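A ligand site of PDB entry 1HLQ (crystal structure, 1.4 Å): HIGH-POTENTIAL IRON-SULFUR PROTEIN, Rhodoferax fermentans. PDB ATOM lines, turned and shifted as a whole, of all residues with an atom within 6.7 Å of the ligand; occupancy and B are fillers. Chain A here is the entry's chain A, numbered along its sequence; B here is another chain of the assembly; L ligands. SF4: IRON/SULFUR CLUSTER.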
ATOM      1  N   LEU A  15       2.661  11.859  -9.658  1.00  0.00           N
ATOM      2  CA  LEU A  15       3.879  12.641  -9.526  1.00  0.00           C
ATOM      3  C   LEU A  15       4.577  12.922 -10.851  1.00  0.00           C
ATOM      4  O   LEU A  15       5.709  13.423 -10.884  1.00  0.00           O
ATOM      5  CB  LEU A  15       4.854  11.923  -8.584  1.00  0.00           C
ATOM      6  CG  LEU A  15       4.435  11.850  -7.121  1.00  0.00           C
ATOM      7  CD1 LEU A  15       5.270  10.869  -6.337  1.00  0.00           C
ATOM      8  CD2 LEU A  15       4.525  13.237  -6.504  1.00  0.00           C
ATOM      9  N   TYR A  17       5.996  10.879 -12.768  1.00  0.00           N
ATOM     10  CA  TYR A  17       7.246  10.132 -12.846  1.00  0.00           C
ATOM     11  C   TYR A  17       7.531   9.638 -14.254  1.00  0.00           C
ATOM     12  O   TYR A  17       6.684   9.103 -14.952  1.00  0.00           O
ATOM     13  CB  TYR A  17       7.180   8.902 -11.917  1.00  0.00           C
ATOM     14  CG  TYR A  17       8.385   7.992 -12.082  1.00  0.00           C
ATOM     15  CD1 TYR A  17       9.584   8.210 -11.424  1.00  0.00           C
ATOM     16  CD2 TYR A  17       8.293   6.865 -12.887  1.00  0.00           C
ATOM     17  CE1 TYR A  17      10.676   7.389 -11.638  1.00  0.00           C
ATOM     18  CE2 TYR A  17       9.364   6.013 -13.106  1.00  0.00           C
ATOM     19  CZ  TYR A  17      10.548   6.272 -12.446  1.00  0.00           C
ATOM     20  OH  TYR A  17      11.641   5.442 -12.624  1.00  0.00           O
ATOM     21  N   VAL A  18       8.804   9.802 -14.631  1.00  0.00           N
ATOM     22  CA  VAL A  18       9.298   9.258 -15.897  1.00  0.00           C
ATOM     23  C   VAL A  18      10.587   8.520 -15.575  1.00  0.00           C
ATOM     24  O   VAL A  18      11.381   8.934 -14.725  1.00  0.00           O
ATOM     25  CB  VAL A  18       9.528  10.297 -17.012  1.00  0.00           C
ATOM     26  CG1 VAL A  18       8.208  10.762 -17.614  1.00  0.00           C
ATOM     27  CG2 VAL A  18      10.356  11.454 -16.489  1.00  0.00           C
ATOM     28  N   GLN A  36      17.885  17.746 -13.154  1.00  0.00           N
ATOM     29  CA  GLN A  36      17.100  17.082 -12.132  1.00  0.00           C
ATOM     30  C   GLN A  36      16.875  15.620 -12.573  1.00  0.00           C
ATOM     31  O   GLN A  36      16.260  15.356 -13.572  1.00  0.00           O
ATOM     32  CB  GLN A  36      15.755  17.770 -11.936  1.00  0.00           C
ATOM     33  CG  GLN A  36      15.865  19.232 -11.572  1.00  0.00           C
ATOM     34  CD  GLN A  36      14.512  19.903 -11.428  1.00  0.00           C
ATOM     35  OE1 GLN A  36      13.447  19.309 -11.537  1.00  0.00           O
ATOM     36  NE2 GLN A  36      14.515  21.209 -11.171  1.00  0.00           N
ATOM     37  N   SER A  37      17.337  14.707 -11.735  1.00  0.00           N
ATOM     38  CA  SER A  37      17.054  13.292 -11.963  1.00  0.00           C
ATOM     39  C   SER A  37      17.051  12.619 -10.599  1.00  0.00           C
ATOM     40  O   SER A  37      17.514  13.166  -9.602  1.00  0.00           O
ATOM     41  CB  SER A  37      18.052  12.632 -12.919  1.00  0.00           C
ATOM     42  OG  SER A  37      19.339  12.719 -12.341  1.00  0.00           O
ATOM     43  N   CYS A  38      16.627  11.356 -10.550  1.00  0.00           N
ATOM     44  CA  CYS A  38      16.663  10.639  -9.270  1.00  0.00           C
ATOM     45  C   CYS A  38      18.082  10.609  -8.724  1.00  0.00           C
ATOM     46  O   CYS A  38      18.294  10.768  -7.535  1.00  0.00           O
ATOM     47  CB  CYS A  38      16.101   9.235  -9.434  1.00  0.00           C
ATOM     48  SG  CYS A  38      14.403   9.176 -10.054  1.00  0.00           S
ATOM     49  N   SER A  39      19.064  10.474  -9.612  1.00  0.00           N
ATOM     50  CA  SER A  39      20.458  10.438  -9.167  1.00  0.00           C
ATOM     51  C   SER A  39      20.875  11.721  -8.459  1.00  0.00           C
ATOM     52  O   SER A  39      21.822  11.666  -7.673  1.00  0.00           O
ATOM     53  CB  SER A  39      21.398  10.170 -10.341  1.00  0.00           C
ATOM     54  OG  SER A  39      21.267  11.189 -11.304  1.00  0.00           O
ATOM     55  N   CYS A  41      18.625  13.654  -6.714  1.00  0.00           N
ATOM     56  CA  CYS A  41      17.546  13.917  -5.779  1.00  0.00           C
ATOM     57  C   CYS A  41      17.894  13.525  -4.347  1.00  0.00           C
ATOM     58  O   CYS A  41      18.462  12.450  -4.110  1.00  0.00           O
ATOM     59  CB  CYS A  41      16.288  13.131  -6.228  1.00  0.00           C
ATOM     60  SG  CYS A  41      14.837  13.364  -5.186  1.00  0.00           S
ATOM     61  N   ALA A  42      17.493  14.344  -3.376  1.00  0.00           N
ATOM     62  CA  ALA A  42      17.764  14.052  -1.979  1.00  0.00           C
ATOM     63  C   ALA A  42      17.056  12.816  -1.472  1.00  0.00           C
ATOM     64  O   ALA A  42      17.423  12.225  -0.450  1.00  0.00           O
ATOM     65  CB  ALA A  42      17.393  15.261  -1.134  1.00  0.00           C
ATOM     66  N   LEU A  43      15.983  12.372  -2.137  1.00  0.00           N
ATOM     67  CA  LEU A  43      15.207  11.220  -1.701  1.00  0.00           C
ATOM     68  C   LEU A  43      15.710   9.906  -2.251  1.00  0.00           C
ATOM     69  O   LEU A  43      15.421   8.855  -1.652  1.00  0.00           O
ATOM     70  CB  LEU A  43      13.718  11.429  -2.032  1.00  0.00           C
ATOM     71  CG  LEU A  43      13.094  12.682  -1.412  1.00  0.00           C
ATOM     72  CD1 LEU A  43      11.621  12.801  -1.789  1.00  0.00           C
ATOM     73  CD2 LEU A  43      13.263  12.719   0.099  1.00  0.00           C
ATOM     74  N   TYR A  44      16.472   9.918  -3.337  1.00  0.00           N
ATOM     75  CA  TYR A  44      16.962   8.684  -3.948  1.00  0.00           C
ATOM     76  C   TYR A  44      17.853   7.906  -2.999  1.00  0.00           C
ATOM     77  O   TYR A  44      18.759   8.480  -2.395  1.00  0.00           O
ATOM     78  CB  TYR A  44      17.691   8.975  -5.245  1.00  0.00           C
ATOM     79  CG  TYR A  44      18.173   7.797  -6.054  1.00  0.00           C
ATOM     80  CD1 TYR A  44      19.513   7.660  -6.370  1.00  0.00           C
ATOM     81  CD2 TYR A  44      17.281   6.834  -6.531  1.00  0.00           C
ATOM     82  CE1 TYR A  44      19.952   6.585  -7.132  1.00  0.00           C
ATOM     83  CE2 TYR A  44      17.724   5.776  -7.289  1.00  0.00           C
ATOM     84  CZ  TYR A  44      19.064   5.653  -7.588  1.00  0.00           C
ATOM     85  OH  TYR A  44      19.525   4.608  -8.346  1.00  0.00           O
ATOM     86  N   GLN A  45      17.631   6.586  -2.925  1.00  0.00           N
ATOM     87  CA  GLN A  45      18.438   5.778  -1.995  1.00  0.00           C
ATOM     88  C   GLN A  45      19.436   4.878  -2.693  1.00  0.00           C
ATOM     89  O   GLN A  45      20.231   4.187  -2.029  1.00  0.00           O
ATOM     90  CB  GLN A  45      17.489   4.927  -1.135  1.00  0.00           C
ATOM     91  CG  GLN A  45      16.421   5.696  -0.405  1.00  0.00           C
ATOM     92  CD  GLN A  45      15.474   4.935   0.485  1.00  0.00           C
ATOM     93  OE1 GLN A  45      14.730   5.532   1.286  1.00  0.00           O
ATOM     94  NE2 GLN A  45      15.460   3.611   0.411  1.00  0.00           N
ATOM     95  N   ALA A  53      15.942   2.465  -4.686  1.00  0.00           N
ATOM     96  CA  ALA A  53      14.696   2.813  -4.024  1.00  0.00           C
ATOM     97  C   ALA A  53      14.463   4.309  -3.851  1.00  0.00           C
ATOM     98  O   ALA A  53      15.381   5.120  -3.729  1.00  0.00           O
ATOM     99  CB  ALA A  53      14.656   2.178  -2.629  1.00  0.00           C
ATOM    100  N   CYS A  54      13.172   4.606  -3.765  1.00  0.00           N
ATOM    101  CA  CYS A  54      12.681   5.962  -3.477  1.00  0.00           C
ATOM    102  C   CYS A  54      11.573   5.807  -2.451  1.00  0.00           C
ATOM    103  O   CYS A  54      10.670   4.980  -2.623  1.00  0.00           O
ATOM    104  CB  CYS A  54      12.172   6.630  -4.748  1.00  0.00           C
ATOM    105  SG  CYS A  54      11.270   8.160  -4.373  1.00  0.00           S
ATOM    106  N   PRO A  55      11.537   6.626  -1.405  1.00  0.00           N
ATOM    107  CA  PRO A  55      10.513   6.515  -0.373  1.00  0.00           C
ATOM    108  C   PRO A  55       9.103   6.697  -0.846  1.00  0.00           C
ATOM    109  O   PRO A  55       8.131   6.272  -0.208  1.00  0.00           O
ATOM    110  CB  PRO A  55      10.925   7.538   0.680  1.00  0.00           C
ATOM    111  CG  PRO A  55      11.768   8.514  -0.077  1.00  0.00           C
ATOM    112  CD  PRO A  55      12.519   7.678  -1.087  1.00  0.00           C
ATOM    113  N   LEU A  56       8.866   7.345  -1.988  1.00  0.00           N
ATOM    114  CA  LEU A  56       7.563   7.589  -2.528  1.00  0.00           C
ATOM    115  C   LEU A  56       7.016   6.405  -3.305  1.00  0.00           C
ATOM    116  O   LEU A  56       5.875   6.492  -3.721  1.00  0.00           O
ATOM    117  CB  LEU A  56       7.561   8.833  -3.441  1.00  0.00           C
ATOM    118  CG  LEU A  56       8.090  10.095  -2.712  1.00  0.00           C
ATOM    119  CD1 LEU A  56       8.090  11.294  -3.647  1.00  0.00           C
ATOM    120  CD2 LEU A  56       7.301  10.384  -1.452  1.00  0.00           C
ATOM    121  N   PHE A  57       7.884   5.423  -3.584  1.00  0.00           N
ATOM    122  CA  PHE A  57       7.489   4.279  -4.407  1.00  0.00           C
ATOM    123  C   PHE A  57       7.777   2.942  -3.733  1.00  0.00           C
ATOM    124  O   PHE A  57       8.769   2.258  -3.954  1.00  0.00           O
ATOM    125  CB  PHE A  57       8.209   4.374  -5.768  1.00  0.00           C
ATOM    126  CG  PHE A  57       7.724   5.547  -6.574  1.00  0.00           C
ATOM    127  CD1 PHE A  57       8.458   6.741  -6.632  1.00  0.00           C
ATOM    128  CD2 PHE A  57       6.509   5.511  -7.233  1.00  0.00           C
ATOM    129  CE1 PHE A  57       7.943   7.818  -7.335  1.00  0.00           C
ATOM    130  CE2 PHE A  57       5.999   6.567  -7.960  1.00  0.00           C
ATOM    131  CZ  PHE A  57       6.750   7.752  -7.997  1.00  0.00           C
ATOM    132  N   VAL A  62      13.187   2.937  -8.691  1.00  0.00           N
ATOM    133  CA  VAL A  62      13.130   3.947  -9.743  1.00  0.00           C
ATOM    134  C   VAL A  62      14.426   3.906 -10.537  1.00  0.00           C
ATOM    135  O   VAL A  62      15.431   3.378 -10.055  1.00  0.00           O
ATOM    136  CB  VAL A  62      12.893   5.362  -9.183  1.00  0.00           C
ATOM    137  CG1 VAL A  62      11.513   5.452  -8.532  1.00  0.00           C
ATOM    138  CG2 VAL A  62      13.980   5.794  -8.205  1.00  0.00           C
ATOM    139  N   VAL A  63      14.425   4.438 -11.743  1.00  0.00           N
ATOM    140  CA  VAL A  63      15.617   4.497 -12.588  1.00  0.00           C
ATOM    141  C   VAL A  63      16.361   5.772 -12.235  1.00  0.00           C
ATOM    142  O   VAL A  63      15.753   6.860 -12.159  1.00  0.00           O
ATOM    143  CB  VAL A  63      15.237   4.444 -14.069  1.00  0.00           C
ATOM    144  CG1 VAL A  63      16.447   4.602 -14.984  1.00  0.00           C
ATOM    145  CG2 VAL A  63      14.565   3.103 -14.346  1.00  0.00           C
ATOM    146  N   ALA A  64      17.680   5.709 -12.055  1.00  0.00           N
ATOM    147  CA  ALA A  64      18.488   6.832 -11.621  1.00  0.00           C
ATOM    148  C   ALA A  64      18.443   8.031 -12.556  1.00  0.00           C
ATOM    149  O   ALA A  64      18.549   9.196 -12.127  1.00  0.00           O
ATOM    150  CB  ALA A  64      19.912   6.370 -11.390  1.00  0.00           C
ATOM    151  N   GLY A  66      15.797   8.863 -14.082  1.00  0.00           N
ATOM    152  CA  GLY A  66      14.419   9.264 -14.010  1.00  0.00           C
ATOM    153  C   GLY A  66      14.151  10.573 -13.281  1.00  0.00           C
ATOM    154  O   GLY A  66      15.062  11.306 -12.908  1.00  0.00           O
ATOM    155  N   TRP A  67      12.876  10.887 -13.081  1.00  0.00           N
ATOM    156  CA  TRP A  67      12.449  12.128 -12.462  1.00  0.00           C
ATOM    157  C   TRP A  67      10.982  12.045 -12.066  1.00  0.00           C
ATOM    158  O   TRP A  67      10.190  11.362 -12.691  1.00  0.00           O
ATOM    159  CB  TRP A  67      12.581  13.265 -13.504  1.00  0.00           C
ATOM    160  CG  TRP A  67      12.217  14.637 -13.011  1.00  0.00           C
ATOM    161  CD1 TRP A  67      13.050  15.531 -12.414  1.00  0.00           C
ATOM    162  CD2 TRP A  67      10.935  15.264 -13.060  1.00  0.00           C
ATOM    163  NE1 TRP A  67      12.369  16.683 -12.072  1.00  0.00           N
ATOM    164  CE2 TRP A  67      11.063  16.538 -12.469  1.00  0.00           C
ATOM    165  CE3 TRP A  67       9.679  14.885 -13.551  1.00  0.00           C
ATOM    166  CZ2 TRP A  67       9.997  17.424 -12.350  1.00  0.00           C
ATOM    167  CZ3 TRP A  67       8.614  15.764 -13.425  1.00  0.00           C
ATOM    168  CH2 TRP A  67       8.787  17.017 -12.845  1.00  0.00           C
ATOM    169  N   CYS A  68      10.653  12.789 -11.013  1.00  0.00           N
ATOM    170  CA  CYS A  68       9.252  12.986 -10.656  1.00  0.00           C
ATOM    171  C   CYS A  68       9.132  14.390 -10.064  1.00  0.00           C
ATOM    172  O   CYS A  68      10.121  15.064  -9.809  1.00  0.00           O
ATOM    173  CB  CYS A  68       8.642  11.931  -9.761  1.00  0.00           C
ATOM    174  SG  CYS A  68       8.905  12.249  -7.991  1.00  0.00           S
ATOM    175  N   SER A  69       7.877  14.825  -9.906  1.00  0.00           N
ATOM    176  CA  SER A  69       7.612  16.197  -9.491  1.00  0.00           C
ATOM    177  C   SER A  69       8.109  16.511  -8.102  1.00  0.00           C
ATOM    178  O   SER A  69       8.242  17.705  -7.764  1.00  0.00           O
ATOM    179  CB  SER A  69       6.080  16.360  -9.564  1.00  0.00           C
ATOM    180  OG  SER A  69       5.639  17.657  -9.237  1.00  0.00           O
ATOM    181  N   ALA A  70       8.375  15.537  -7.259  1.00  0.00           N
ATOM    182  CA  ALA A  70       8.920  15.720  -5.934  1.00  0.00           C
ATOM    183  C   ALA A  70      10.433  15.875  -5.917  1.00  0.00           C
ATOM    184  O   ALA A  70      11.029  15.934  -4.836  1.00  0.00           O
ATOM    185  CB  ALA A  70       8.526  14.547  -5.027  1.00  0.00           C
ATOM    186  N   TRP A  71      11.077  15.900  -7.111  1.00  0.00           N
ATOM    187  CA  TRP A  71      12.520  16.023  -7.146  1.00  0.00           C
ATOM    188  C   TRP A  71      13.013  17.046  -6.126  1.00  0.00           C
ATOM    189  O   TRP A  71      12.553  18.191  -6.185  1.00  0.00           O
ATOM    190  CB  TRP A  71      13.012  16.369  -8.548  1.00  0.00           C
ATOM    191  CG  TRP A  71      14.505  16.472  -8.577  1.00  0.00           C
ATOM    192  CD1 TRP A  71      15.373  15.451  -8.794  1.00  0.00           C
ATOM    193  CD2 TRP A  71      15.294  17.648  -8.391  1.00  0.00           C
ATOM    194  NE1 TRP A  71      16.670  15.895  -8.710  1.00  0.00           N
ATOM    195  CE2 TRP A  71      16.645  17.253  -8.486  1.00  0.00           C
ATOM    196  CE3 TRP A  71      14.982  18.994  -8.147  1.00  0.00           C
ATOM    197  CZ2 TRP A  71      17.703  18.150  -8.339  1.00  0.00           C
ATOM    198  CZ3 TRP A  71      16.042  19.869  -8.012  1.00  0.00           C
ATOM    199  CH2 TRP A  71      17.371  19.444  -8.111  1.00  0.00           C
ATOM    200  N   ALA A  72      13.894  16.612  -5.248  1.00  0.00           N
ATOM    201  CA  ALA A  72      14.300  17.428  -4.116  1.00  0.00           C
ATOM    202  C   ALA A  72      15.770  17.772  -4.183  1.00  0.00           C
ATOM    203  O   ALA A  72      16.605  16.888  -4.096  1.00  0.00           O
ATOM    204  CB  ALA A  72      13.933  16.673  -2.847  1.00  0.00           C
ATOM    205  N   ALA B  70      10.852  19.097  -1.537  1.00  0.00           N
ATOM    206  CA  ALA B  70      10.186  18.050  -2.304  1.00  0.00           C
ATOM    207  C   ALA B  70       8.798  18.472  -2.786  1.00  0.00           C
ATOM    208  O   ALA B  70       8.071  17.668  -3.385  1.00  0.00           O
ATOM    209  CB  ALA B  70      10.047  16.752  -1.501  1.00  0.00           C
HETATM  210 FE1  SF4 L   1      13.240  10.160  -8.348  1.00  0.00          FE
HETATM  211 FE2  SF4 L   1      13.350  11.922  -6.249  1.00  0.00          FE
HETATM  212 FE3  SF4 L   1      11.996   9.594  -6.017  1.00  0.00          FE
HETATM  213 FE4  SF4 L   1      11.065  11.557  -7.622  1.00  0.00          FE
HETATM  214  S1  SF4 L   1      11.318  11.728  -5.341  1.00  0.00           S
HETATM  215  S2  SF4 L   1      11.174   9.300  -8.191  1.00  0.00           S
HETATM  216  S3  SF4 L   1      12.992  12.478  -8.470  1.00  0.00           S
HETATM  217  S4  SF4 L   1      14.247   9.743  -6.310  1.00  0.00           S
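The indole nitrogen (NE1) of Trp 71 is in hydrogen-bond range of the backbone carbonyl oxygen (O) of Ser 37 (3.0 Å).
The backbone carbonyl oxygen of Val 63 sits close to the side-chain sulfur of Cys 38 (3.4 Å).
The backbone NH of Leu 56 sits close to the side-chain sulfur of Cys 54, 3.5 Å away.
The side-chain sulfur of Cys 41 sits close to the backbone NH of Leu 43, at 3.4 Å.
The side-chain sulfur of Cys 38 lies close to the backbone NH of Trp 67, 3.8 Å away.
The side-chain sulfur (SG) of Cys 41 lies close to the backbone NH (N) of Ala 72 (3.4 Å).
The backbone NH (N) of Ala 70 of chain A lies close to the side-chain sulfur (SG) of Cys 68 (3.4 Å).
N of Cys 38 is in hydrogen-bond range of O of Gly 66, 2.8 Å away.
N of Tyr 44 sits close to S4 of the ligand.
The side-chain sulfur (SG) of Cys 54 is bound to an iron atom (FE3) of the ligand (2.3 Å).
The side-chain sulfur of Cys 38 is bound to an iron atom (FE1) of the ligand (2.3 Å).
S3 of the ligand lies close to N of Cys 68, at 3.5 Å.
The side-chain sulfur (SG) of Cys 41 is bound to an iron atom (FE2) of the ligand, at 2.3 Å.
SG of Cys 68 is bound to FE4 of the ligand, at 2.3 Å.
Merely in contact with the ligand: Phe 57, Leu 56, Leu 43, Tyr 17, Trp 71, Val 62 and Ala 70 of chain A.
12 residues have an atom within 4 Å of the ligand: Tyr 17, Cys 38, Cys 41, Leu 43, Tyr 44, Cys 54, Leu 56, Phe 57, Val 62, Cys 68, Ala 70 of chain A and Trp 71.
The nearest printed residue that does not touch the ligand is Trp 67 (4.04 Å).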
